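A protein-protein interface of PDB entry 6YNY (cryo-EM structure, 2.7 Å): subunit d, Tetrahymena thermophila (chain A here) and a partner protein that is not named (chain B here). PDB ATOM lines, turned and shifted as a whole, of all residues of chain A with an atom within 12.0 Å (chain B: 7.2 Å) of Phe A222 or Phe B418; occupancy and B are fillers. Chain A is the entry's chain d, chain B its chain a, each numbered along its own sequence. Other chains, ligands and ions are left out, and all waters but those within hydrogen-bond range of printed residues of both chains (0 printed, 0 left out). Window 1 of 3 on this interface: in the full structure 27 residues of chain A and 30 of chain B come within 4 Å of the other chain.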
ATOM      1  N   ASN A 186      11.599 -25.418   3.244  1.00  0.00           N
ATOM      2  CA  ASN A 186      12.583 -24.500   3.811  1.00  0.00           C
ATOM      3  C   ASN A 186      13.229 -23.690   2.690  1.00  0.00           C
ATOM      4  O   ASN A 186      14.440 -23.707   2.472  1.00  0.00           O
ATOM      5  CB  ASN A 186      13.620 -25.266   4.622  1.00  0.00           C
ATOM      6  CG  ASN A 186      13.134 -25.614   6.007  1.00  0.00           C
ATOM      7  OD1 ASN A 186      13.213 -24.804   6.928  1.00  0.00           O
ATOM      8  ND2 ASN A 186      12.632 -26.827   6.167  1.00  0.00           N
ATOM      9  N   ILE A 188      13.649 -20.584   2.397  1.00  0.00           N
ATOM     10  CA  ILE A 188      14.353 -19.369   2.794  1.00  0.00           C
ATOM     11  C   ILE A 188      15.849 -19.670   2.726  1.00  0.00           C
ATOM     12  O   ILE A 188      16.330 -20.513   3.500  1.00  0.00           O
ATOM     13  CB  ILE A 188      13.944 -18.906   4.195  1.00  0.00           C
ATOM     14  CG1 ILE A 188      12.441 -18.645   4.244  1.00  0.00           C
ATOM     15  CG2 ILE A 188      14.703 -17.660   4.563  1.00  0.00           C
ATOM     16  CD1 ILE A 188      11.928 -18.279   5.607  1.00  0.00           C
ATOM     17  N   ILE A 212      18.655 -14.270   8.152  1.00  0.00           N
ATOM     18  CA  ILE A 212      17.557 -15.102   8.611  1.00  0.00           C
ATOM     19  C   ILE A 212      17.988 -15.868   9.850  1.00  0.00           C
ATOM     20  O   ILE A 212      19.147 -16.287   9.976  1.00  0.00           O
ATOM     21  CB  ILE A 212      17.100 -16.054   7.494  1.00  0.00           C
ATOM     22  CG1 ILE A 212      15.727 -16.635   7.820  1.00  0.00           C
ATOM     23  CG2 ILE A 212      18.099 -17.165   7.296  1.00  0.00           C
ATOM     24  CD1 ILE A 212      14.607 -15.656   7.640  1.00  0.00           C
ATOM     25  N   SER A 213      17.059 -16.040  10.782  1.00  0.00           N
ATOM     26  CA  SER A 213      17.357 -16.782  11.993  1.00  0.00           C
ATOM     27  C   SER A 213      17.535 -18.262  11.679  1.00  0.00           C
ATOM     28  O   SER A 213      16.976 -18.791  10.716  1.00  0.00           O
ATOM     29  CB  SER A 213      16.252 -16.581  13.025  1.00  0.00           C
ATOM     30  OG  SER A 213      14.976 -16.808  12.465  1.00  0.00           O
ATOM     31  N   PHE A 214      18.326 -18.926  12.511  1.00  0.00           N
ATOM     32  CA  PHE A 214      18.724 -20.301  12.248  1.00  0.00           C
ATOM     33  C   PHE A 214      17.524 -21.240  12.283  1.00  0.00           C
ATOM     34  O   PHE A 214      16.745 -21.242  13.239  1.00  0.00           O
ATOM     35  CB  PHE A 214      19.773 -20.721  13.276  1.00  0.00           C
ATOM     36  CG  PHE A 214      20.533 -21.956  12.913  1.00  0.00           C
ATOM     37  CD1 PHE A 214      20.724 -22.956  13.840  1.00  0.00           C
ATOM     38  CD2 PHE A 214      21.065 -22.115  11.652  1.00  0.00           C
ATOM     39  CE1 PHE A 214      21.425 -24.086  13.517  1.00  0.00           C
ATOM     40  CE2 PHE A 214      21.764 -23.246  11.324  1.00  0.00           C
ATOM     41  CZ  PHE A 214      21.945 -24.233  12.258  1.00  0.00           C
ATOM     42  N   TYR A 215      17.384 -22.041  11.225  1.00  0.00           N
ATOM     43  CA  TYR A 215      16.316 -23.037  11.110  1.00  0.00           C
ATOM     44  C   TYR A 215      14.934 -22.388  11.096  1.00  0.00           C
ATOM     45  O   TYR A 215      13.963 -22.935  11.621  1.00  0.00           O
ATOM     46  CB  TYR A 215      16.417 -24.082  12.222  1.00  0.00           C
ATOM     47  CG  TYR A 215      17.239 -25.284  11.839  1.00  0.00           C
ATOM     48  CD1 TYR A 215      16.644 -26.516  11.638  1.00  0.00           C
ATOM     49  CD2 TYR A 215      18.607 -25.186  11.662  1.00  0.00           C
ATOM     50  CE1 TYR A 215      17.388 -27.615  11.285  1.00  0.00           C
ATOM     51  CE2 TYR A 215      19.357 -26.279  11.308  1.00  0.00           C
ATOM     52  CZ  TYR A 215      18.742 -27.491  11.120  1.00  0.00           C
ATOM     53  OH  TYR A 215      19.489 -28.587  10.767  1.00  0.00           O
ATOM     54  N   ARG A 216      14.841 -21.220  10.475  1.00  0.00           N
ATOM     55  CA  ARG A 216      13.573 -20.518  10.360  1.00  0.00           C
ATOM     56  C   ARG A 216      12.763 -21.084   9.203  1.00  0.00           C
ATOM     57  O   ARG A 216      13.249 -21.159   8.072  1.00  0.00           O
ATOM     58  CB  ARG A 216      13.818 -19.025  10.159  1.00  0.00           C
ATOM     59  CG  ARG A 216      12.568 -18.196   9.967  1.00  0.00           C
ATOM     60  CD  ARG A 216      11.683 -18.248  11.179  1.00  0.00           C
ATOM     61  NE  ARG A 216      10.544 -17.345  11.061  1.00  0.00           N
ATOM     62  CZ  ARG A 216      10.563 -16.064  11.413  1.00  0.00           C
ATOM     63  NH1 ARG A 216      11.664 -15.515  11.908  1.00  0.00           N
ATOM     64  NH2 ARG A 216       9.474 -15.329  11.270  1.00  0.00           N
ATOM     65  N   HIS A 217      11.528 -21.483   9.491  1.00  0.00           N
ATOM     66  CA  HIS A 217      10.640 -21.997   8.462  1.00  0.00           C
ATOM     67  C   HIS A 217       9.664 -20.917   8.012  1.00  0.00           C
ATOM     68  O   HIS A 217       9.170 -20.146   8.838  1.00  0.00           O
ATOM     69  CB  HIS A 217       9.860 -23.204   8.980  1.00  0.00           C
ATOM     70  CG  HIS A 217       9.244 -24.035   7.901  1.00  0.00           C
ATOM     71  ND1 HIS A 217       8.014 -23.752   7.353  1.00  0.00           N
ATOM     72  CD2 HIS A 217       9.692 -25.144   7.270  1.00  0.00           C
ATOM     73  CE1 HIS A 217       7.732 -24.648   6.425  1.00  0.00           C
ATOM     74  NE2 HIS A 217       8.732 -25.507   6.359  1.00  0.00           N
ATOM     75  N   PRO A 218       9.361 -20.825   6.713  1.00  0.00           N
ATOM     76  CA  PRO A 218       8.440 -19.784   6.240  1.00  0.00           C
ATOM     77  C   PRO A 218       7.006 -19.948   6.712  1.00  0.00           C
ATOM     78  O   PRO A 218       6.175 -19.085   6.409  1.00  0.00           O
ATOM     79  CB  PRO A 218       8.531 -19.907   4.713  1.00  0.00           C
ATOM     80  CG  PRO A 218       9.070 -21.248   4.461  1.00  0.00           C
ATOM     81  CD  PRO A 218       9.953 -21.577   5.597  1.00  0.00           C
ATOM     82  N   ALA A 219       6.686 -21.013   7.441  1.00  0.00           N
ATOM     83  CA  ALA A 219       5.331 -21.261   7.903  1.00  0.00           C
ATOM     84  C   ALA A 219       5.159 -21.094   9.402  1.00  0.00           C
ATOM     85  O   ALA A 219       4.025 -20.941   9.862  1.00  0.00           O
ATOM     86  CB  ALA A 219       4.886 -22.675   7.516  1.00  0.00           C
ATOM     87  N   ASP A 220       6.243 -21.129  10.167  1.00  0.00           N
ATOM     88  CA  ASP A 220       6.140 -20.988  11.610  1.00  0.00           C
ATOM     89  C   ASP A 220       5.719 -19.574  11.982  1.00  0.00           C
ATOM     90  O   ASP A 220       6.159 -18.593  11.375  1.00  0.00           O
ATOM     91  CB  ASP A 220       7.471 -21.340  12.274  1.00  0.00           C
ATOM     92  CG  ASP A 220       8.613 -20.462  11.810  1.00  0.00           C
ATOM     93  OD1 ASP A 220       8.554 -19.234  12.032  1.00  0.00           O
ATOM     94  OD2 ASP A 220       9.583 -21.002  11.240  1.00  0.00           O
ATOM     95  N   ASP A 221       4.851 -19.475  12.984  1.00  0.00           N
ATOM     96  CA  ASP A 221       4.343 -18.192  13.462  1.00  0.00           C
ATOM     97  C   ASP A 221       4.195 -18.293  14.972  1.00  0.00           C
ATOM     98  O   ASP A 221       3.294 -18.975  15.466  1.00  0.00           O
ATOM     99  CB  ASP A 221       3.013 -17.838  12.799  1.00  0.00           C
ATOM    100  CG  ASP A 221       2.555 -16.430  13.122  1.00  0.00           C
ATOM    101  OD1 ASP A 221       3.020 -15.862  14.131  1.00  0.00           O
ATOM    102  OD2 ASP A 221       1.722 -15.889  12.368  1.00  0.00           O
ATOM    103  N   PHE A 222       5.079 -17.614  15.701  1.00  0.00           N
ATOM    104  CA  PHE A 222       5.082 -17.625  17.156  1.00  0.00           C
ATOM    105  C   PHE A 222       4.399 -16.400  17.750  1.00  0.00           C
ATOM    106  O   PHE A 222       4.585 -16.108  18.935  1.00  0.00           O
ATOM    107  CB  PHE A 222       6.514 -17.726  17.675  1.00  0.00           C
ATOM    108  CG  PHE A 222       7.144 -19.070  17.471  1.00  0.00           C
ATOM    109  CD1 PHE A 222       7.369 -19.910  18.543  1.00  0.00           C
ATOM    110  CD2 PHE A 222       7.515 -19.494  16.209  1.00  0.00           C
ATOM    111  CE1 PHE A 222       7.952 -21.141  18.362  1.00  0.00           C
ATOM    112  CE2 PHE A 222       8.096 -20.727  16.025  1.00  0.00           C
ATOM    113  CZ  PHE A 222       8.314 -21.550  17.103  1.00  0.00           C
ATOM    114  N   LYS A 223       3.615 -15.679  16.955  1.00  0.00           N
ATOM    115  CA  LYS A 223       2.934 -14.495  17.458  1.00  0.00           C
ATOM    116  C   LYS A 223       2.033 -14.848  18.631  1.00  0.00           C
ATOM    117  O   LYS A 223       1.343 -15.870  18.625  1.00  0.00           O
ATOM    118  CB  LYS A 223       2.108 -13.840  16.354  1.00  0.00           C
ATOM    119  CG  LYS A 223       2.876 -12.872  15.491  1.00  0.00           C
ATOM    120  CD  LYS A 223       3.225 -11.616  16.258  1.00  0.00           C
ATOM    121  CE  LYS A 223       3.940 -10.622  15.379  1.00  0.00           C
ATOM    122  NZ  LYS A 223       3.075 -10.145  14.277  1.00  0.00           N
ATOM    123  N   CYS A 224       2.044 -13.987  19.637  1.00  0.00           N
ATOM    124  CA  CYS A 224       1.212 -14.119  20.818  1.00  0.00           C
ATOM    125  C   CYS A 224       0.246 -12.941  20.878  1.00  0.00           C
ATOM    126  O   CYS A 224       0.259 -12.051  20.026  1.00  0.00           O
ATOM    127  CB  CYS A 224       2.070 -14.194  22.082  1.00  0.00           C
ATOM    128  SG  CYS A 224       3.369 -15.438  22.032  1.00  0.00           S
ATOM    129  N   ALA A 225      -0.599 -12.942  21.903  1.00  0.00           N
ATOM    130  CA  ALA A 225      -1.559 -11.869  22.099  1.00  0.00           C
ATOM    131  C   ALA A 225      -2.106 -11.957  23.511  1.00  0.00           C
ATOM    132  O   ALA A 225      -2.410 -13.050  23.992  1.00  0.00           O
ATOM    133  CB  ALA A 225      -2.699 -11.955  21.083  1.00  0.00           C
ATOM    134  N   LYS A 226      -2.228 -10.807  24.167  1.00  0.00           N
ATOM    135  CA  LYS A 226      -2.716 -10.756  25.533  1.00  0.00           C
ATOM    136  C   LYS A 226      -3.652  -9.571  25.700  1.00  0.00           C
ATOM    137  O   LYS A 226      -3.639  -8.620  24.916  1.00  0.00           O
ATOM    138  CB  LYS A 226      -1.568 -10.662  26.541  1.00  0.00           C
ATOM    139  CG  LYS A 226      -0.777  -9.386  26.465  1.00  0.00           C
ATOM    140  CD  LYS A 226       0.324  -9.373  27.498  1.00  0.00           C
ATOM    141  CE  LYS A 226       1.130  -8.107  27.427  1.00  0.00           C
ATOM    142  NZ  LYS A 226       2.194  -8.092  28.448  1.00  0.00           N
ATOM    143  N   ALA A 227      -4.474  -9.653  26.740  1.00  0.00           N
ATOM    144  CA  ALA A 227      -5.390  -8.592  27.123  1.00  0.00           C
ATOM    145  C   ALA A 227      -5.067  -8.148  28.538  1.00  0.00           C
ATOM    146  O   ALA A 227      -4.940  -8.982  29.440  1.00  0.00           O
ATOM    147  CB  ALA A 227      -6.838  -9.057  27.036  1.00  0.00           C
ATOM    148  N   THR A 228      -4.927  -6.845  28.727  1.00  0.00           N
ATOM    149  CA  THR A 228      -4.593  -6.264  30.015  1.00  0.00           C
ATOM    150  C   THR A 228      -5.674  -5.276  30.433  1.00  0.00           C
ATOM    151  O   THR A 228      -6.676  -5.080  29.743  1.00  0.00           O
ATOM    152  CB  THR A 228      -3.231  -5.573  29.963  1.00  0.00           C
ATOM    153  OG1 THR A 228      -3.283  -4.481  29.038  1.00  0.00           O
ATOM    154  CG2 THR A 228      -2.162  -6.539  29.524  1.00  0.00           C
ATOM    155  N   LEU A 232      -4.524  -2.054  23.992  1.00  0.00           N
ATOM    156  CA  LEU A 232      -3.424  -2.477  23.133  1.00  0.00           C
ATOM    157  C   LEU A 232      -2.475  -3.423  23.858  1.00  0.00           C
ATOM    158  O   LEU A 232      -1.294  -3.516  23.518  1.00  0.00           O
ATOM    159  CB  LEU A 232      -2.662  -1.268  22.591  1.00  0.00           C
ATOM    160  CG  LEU A 232      -3.552  -0.196  21.965  1.00  0.00           C
ATOM    161  CD1 LEU A 232      -2.743   1.021  21.579  1.00  0.00           C
ATOM    162  CD2 LEU A 232      -4.284  -0.746  20.768  1.00  0.00           C
ATOM    163  N   GLY A 233      -2.983  -4.133  24.861  1.00  0.00           N
ATOM    164  CA  GLY A 233      -2.165  -5.082  25.582  1.00  0.00           C
ATOM    165  C   GLY A 233      -1.060  -4.468  26.402  1.00  0.00           C
ATOM    166  O   GLY A 233      -0.123  -5.170  26.787  1.00  0.00           O
ATOM    167  N   ARG A 234      -1.140  -3.174  26.685  1.00  0.00           N
ATOM    168  CA  ARG A 234      -0.133  -2.504  27.492  1.00  0.00           C
ATOM    169  C   ARG A 234      -0.561  -2.440  28.952  1.00  0.00           C
ATOM    170  O   ARG A 234      -0.509  -3.438  29.671  1.00  0.00           O
ATOM    171  CB  ARG A 234       0.131  -1.097  26.961  1.00  0.00           C
ATOM    172  CG  ARG A 234       1.199  -1.028  25.888  1.00  0.00           C
ATOM    173  CD  ARG A 234       0.784  -1.737  24.628  1.00  0.00           C
ATOM    174  NE  ARG A 234       1.842  -1.725  23.627  1.00  0.00           N
ATOM    175  CZ  ARG A 234       1.721  -2.238  22.410  1.00  0.00           C
ATOM    176  NH1 ARG A 234       0.587  -2.804  22.035  1.00  0.00           N
ATOM    177  NH2 ARG A 234       2.736  -2.185  21.566  1.00  0.00           N
ATOM    178  N   GLU B 222      11.760 -11.932   9.417  1.00  0.00           N
ATOM    179  CA  GLU B 222      12.220 -11.549  10.743  1.00  0.00           C
ATOM    180  C   GLU B 222      11.519 -10.304  11.262  1.00  0.00           C
ATOM    181  O   GLU B 222      11.604 -10.018  12.460  1.00  0.00           O
ATOM    182  CB  GLU B 222      13.730 -11.325  10.724  1.00  0.00           C
ATOM    183  CG  GLU B 222      14.522 -12.541  10.309  1.00  0.00           C
ATOM    184  CD  GLU B 222      14.389 -13.690  11.289  1.00  0.00           C
ATOM    185  OE1 GLU B 222      14.052 -13.434  12.463  1.00  0.00           O
ATOM    186  OE2 GLU B 222      14.618 -14.849  10.888  1.00  0.00           O
ATOM    187  N   LYS B 223      10.842  -9.550  10.396  1.00  0.00           N
ATOM    188  CA  LYS B 223      10.015  -8.448  10.871  1.00  0.00           C
ATOM    189  C   LYS B 223       8.792  -8.943  11.625  1.00  0.00           C
ATOM    190  O   LYS B 223       8.147  -8.155  12.323  1.00  0.00           O
ATOM    191  CB  LYS B 223       9.584  -7.561   9.705  1.00  0.00           C
ATOM    192  CG  LYS B 223      10.716  -6.835   8.995  1.00  0.00           C
ATOM    193  CD  LYS B 223      11.529  -5.944   9.922  1.00  0.00           C
ATOM    194  CE  LYS B 223      10.709  -4.811  10.510  1.00  0.00           C
ATOM    195  NZ  LYS B 223      11.497  -4.047  11.502  1.00  0.00           N
ATOM    196  N   GLU B 224       8.460 -10.226  11.494  1.00  0.00           N
ATOM    197  CA  GLU B 224       7.399 -10.854  12.276  1.00  0.00           C
ATOM    198  C   GLU B 224       6.033 -10.259  11.951  1.00  0.00           C
ATOM    199  O   GLU B 224       5.301  -9.803  12.830  1.00  0.00           O
ATOM    200  CB  GLU B 224       7.698 -10.752  13.769  1.00  0.00           C
ATOM    201  CG  GLU B 224       9.028 -11.353  14.169  1.00  0.00           C
ATOM    202  CD  GLU B 224       9.125 -12.833  13.864  1.00  0.00           C
ATOM    203  OE1 GLU B 224       8.083 -13.454  13.569  1.00  0.00           O
ATOM    204  OE2 GLU B 224      10.246 -13.375  13.918  1.00  0.00           O
ATOM    205  N   ILE B 225       5.698 -10.256  10.666  1.00  0.00           N
ATOM    206  CA  ILE B 225       4.347  -9.894  10.251  1.00  0.00           C
ATOM    207  C   ILE B 225       3.407 -11.075  10.443  1.00  0.00           C
ATOM    208  O   ILE B 225       2.461 -11.023  11.237  1.00  0.00           O
ATOM    209  CB  ILE B 225       4.353  -9.413   8.790  1.00  0.00           C
ATOM    210  CG1 ILE B 225       5.386  -8.305   8.592  1.00  0.00           C
ATOM    211  CG2 ILE B 225       2.983  -8.929   8.381  1.00  0.00           C
ATOM    212  CD1 ILE B 225       5.208  -7.119   9.504  1.00  0.00           C
ATOM    213  N   SER B 227       3.130 -15.614   8.833  1.00  0.00           N
ATOM    214  CA  SER B 227       3.762 -16.643   8.022  1.00  0.00           C
ATOM    215  C   SER B 227       3.991 -16.136   6.605  1.00  0.00           C
ATOM    216  O   SER B 227       3.036 -15.850   5.877  1.00  0.00           O
ATOM    217  CB  SER B 227       2.898 -17.898   8.002  1.00  0.00           C
ATOM    218  OG  SER B 227       2.751 -18.425   9.305  1.00  0.00           O
ATOM    219  N   THR B 416      -0.501  -7.474  18.664  1.00  0.00           N
ATOM    220  CA  THR B 416       0.226  -8.722  18.821  1.00  0.00           C
ATOM    221  C   THR B 416       1.583  -8.439  19.445  1.00  0.00           C
ATOM    222  O   THR B 416       2.081  -7.312  19.414  1.00  0.00           O
ATOM    223  CB  THR B 416       0.418  -9.448  17.487  1.00  0.00           C
ATOM    224  OG1 THR B 416       1.276  -8.681  16.637  1.00  0.00           O
ATOM    225  CG2 THR B 416      -0.910  -9.662  16.795  1.00  0.00           C
ATOM    226  N   PHE B 417       2.178  -9.479  20.015  1.00  0.00           N
ATOM    227  CA  PHE B 417       3.471  -9.355  20.667  1.00  0.00           C
ATOM    228  C   PHE B 417       4.068 -10.745  20.831  1.00  0.00           C
ATOM    229  O   PHE B 417       3.453 -11.754  20.479  1.00  0.00           O
ATOM    230  CB  PHE B 417       3.339  -8.648  22.016  1.00  0.00           C
ATOM    231  CG  PHE B 417       2.985  -9.563  23.144  1.00  0.00           C
ATOM    232  CD1 PHE B 417       1.789 -10.247  23.149  1.00  0.00           C
ATOM    233  CD2 PHE B 417       3.850  -9.734  24.205  1.00  0.00           C
ATOM    234  CE1 PHE B 417       1.468 -11.089  24.183  1.00  0.00           C
ATOM    235  CE2 PHE B 417       3.530 -10.573  25.241  1.00  0.00           C
ATOM    236  CZ  PHE B 417       2.339 -11.250  25.230  1.00  0.00           C
ATOM    237  N   PHE B 418       5.282 -10.784  21.367  1.00  0.00           N
ATOM    238  CA  PHE B 418       5.979 -12.018  21.689  1.00  0.00           C
ATOM    239  C   PHE B 418       6.347 -12.011  23.164  1.00  0.00           C
ATOM    240  O   PHE B 418       6.756 -10.980  23.705  1.00  0.00           O
ATOM    241  CB  PHE B 418       7.238 -12.183  20.842  1.00  0.00           C
ATOM    242  CG  PHE B 418       6.969 -12.307  19.377  1.00  0.00           C
ATOM    243  CD1 PHE B 418       6.639 -13.526  18.824  1.00  0.00           C
ATOM    244  CD2 PHE B 418       7.054 -11.207  18.550  1.00  0.00           C
ATOM    245  CE1 PHE B 418       6.394 -13.643  17.481  1.00  0.00           C
ATOM    246  CE2 PHE B 418       6.810 -11.322  17.207  1.00  0.00           C
ATOM    247  CZ  PHE B 418       6.480 -12.543  16.672  1.00  0.00           C
ATOM    248  N   ILE B 419       6.205 -13.156  23.809  1.00  0.00           N
ATOM    249  CA  ILE B 419       6.516 -13.256  25.227  1.00  0.00           C
ATOM    250  C   ILE B 419       8.019 -13.390  25.415  1.00  0.00           C
ATOM    251  O   ILE B 419       8.727 -13.987  24.599  1.00  0.00           O
ATOM    252  CB  ILE B 419       5.765 -14.435  25.877  1.00  0.00           C
ATOM    253  CG1 ILE B 419       6.198 -15.767  25.266  1.00  0.00           C
ATOM    254  CG2 ILE B 419       4.277 -14.256  25.719  1.00  0.00           C
ATOM    255  CD1 ILE B 419       5.705 -16.962  26.026  1.00  0.00           C
ATOM    256  N   ILE B 420       8.510 -12.812  26.510  1.00  0.00           N
ATOM    257  CA  ILE B 420       9.906 -12.967  26.895  1.00  0.00           C
ATOM    258  C   ILE B 420      10.121 -14.192  27.774  1.00  0.00           C
ATOM    259  O   ILE B 420      11.255 -14.684  27.872  1.00  0.00           O
ATOM    260  CB  ILE B 420      10.392 -11.704  27.626  1.00  0.00           C
ATOM    261  CG1 ILE B 420      11.914 -11.669  27.719  1.00  0.00           C
ATOM    262  CG2 ILE B 420       9.801 -11.644  29.011  1.00  0.00           C
ATOM    263  CD1 ILE B 420      12.590 -11.400  26.425  1.00  0.00           C
ATOM    264  N   GLU B 421       9.071 -14.700  28.409  1.00  0.00           N
ATOM    265  CA  GLU B 421       9.190 -15.864  29.271  1.00  0.00           C
ATOM    266  C   GLU B 421       9.275 -17.135  28.441  1.00  0.00           C
ATOM    267  O   GLU B 421       8.729 -17.222  27.339  1.00  0.00           O
ATOM    268  CB  GLU B 421       7.998 -15.965  30.223  1.00  0.00           C
ATOM    269  CG  GLU B 421       7.781 -14.754  31.104  1.00  0.00           C
ATOM    270  CD  GLU B 421       7.042 -13.631  30.402  1.00  0.00           C
ATOM    271  OE1 GLU B 421       6.564 -13.846  29.268  1.00  0.00           O
ATOM    272  OE2 GLU B 421       6.940 -12.533  30.984  1.00  0.00           O
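The side-chain hydroxyl (OG) of Ser B227 sits at hydrogen-bond distance from the backbone carbonyl oxygen (O) of Ala A219, at 2.9 Å. The guanidinium group (NH1) of Arg A216 is in salt-bridge range of the side-chain carboxylate (OE2) of Glu B224 (3.3 Å). The side-chain carboxylate (OE2) of Glu B222 is in salt-bridge range of the guanidinium group (NH1) of Arg A216 (3.2 Å). The backbone carbonyl oxygen of Glu B224 sits at hydrogen-bond distance from the side-chain amino group of Lys A223 (2.7 Å). O of Ile B225 is in hydrogen-bond range of NZ of Lys A223. O of Phe B417 is in hydrogen-bond range of N of Cys A224. The side-chain amino group (NZ) of Lys A223 is in hydrogen-bond range of the side-chain hydroxyl (OG1) of Thr B416, 3.3 Å away. OE2 of Glu B222 sits at hydrogen-bond distance from OG of Ser A213, at 2.5 Å.
The side-chain carboxylate (OD2) of Asp A220 lies within hydrogen-bond range of the backbone NH (N) of His A217 (2.7 Å). A ring nitrogen (ND1) of His A217 sits close to the backbone NH of Ala A219 (3.0 Å). The side-chain sulfur (SG) of Cys A224 is in hydrogen-bond range of the backbone carbonyl oxygen (O) of Phe A222, at 3.4 Å. The side-chain carboxylate (OD1) of Asp A221 sits at hydrogen-bond distance from the backbone NH (N) of Lys A223. The side-chain carboxylate (OD1) of Asp A220 is in salt-bridge range of the guanidinium group (NE) of Arg A216 (2.9 Å).
Among the printed residues, merely in contact across the chains: Phe A222 with Phe B418 (3.3 Å), Ile A212 with Glu B222 (3.3 Å), Lys A223 with Phe B418 (3.4 Å), Cys A224 with Thr B416 (3.5 Å), Asp A221 with Ser B227 (3.6 Å), Lys A226 with Phe B417 (3.6 Å), Ala A225 with Phe B417 (3.6 Å), Pro A218 with Ser B227 (3.7 Å), Lys A223 with Phe B417 (3.9 Å), Cys A224 with Ile B419 (3.98 Å) and Asp A220 with Ser B227 (3.99 Å).
Phe A222 touches just one residue of chain B: Phe B418 (3.3 Å). Of chain A, only Arg A216 (3.3 Å) and Lys A223 (2.7 Å) come within 4 Å of Glu B224. No residue of chain A comes within 4 Å of Ile B420. Printed residues of chain B within 4 Å of Asp A220: Ser B227. Of the printed residues of chain B, Lys A226 touches Phe B417 (3.6 Å). Of the printed residues of chain B, Lys A223 touches Glu B224, Ile B225, Thr B416, Phe B417 and Phe B418.
Of the 11 printed residues of chain B, 8 touch a printed residue of chain A. Printed residues of chain B that touch a printed residue of chain A: Glu B222, Glu B224, Ile B225, Ser B227, Thr B416, Phe B417, Phe B418 and Ile B419. Of the 22 printed residues of chain A, 12 touch a printed residue of chain B. Hydrophobic or aromatic side chains of chain A within 4 Å of the printed part of chain B: Ile A212. Among the printed residues, 19 pairs touch across the chains. Among the printed residues, Asp or Glu carboxylates within 4 Å of a Lys or Arg side-chain nitrogen of the other chain: Arg A216 with Glu B222 and Arg A216 with Glu B224.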
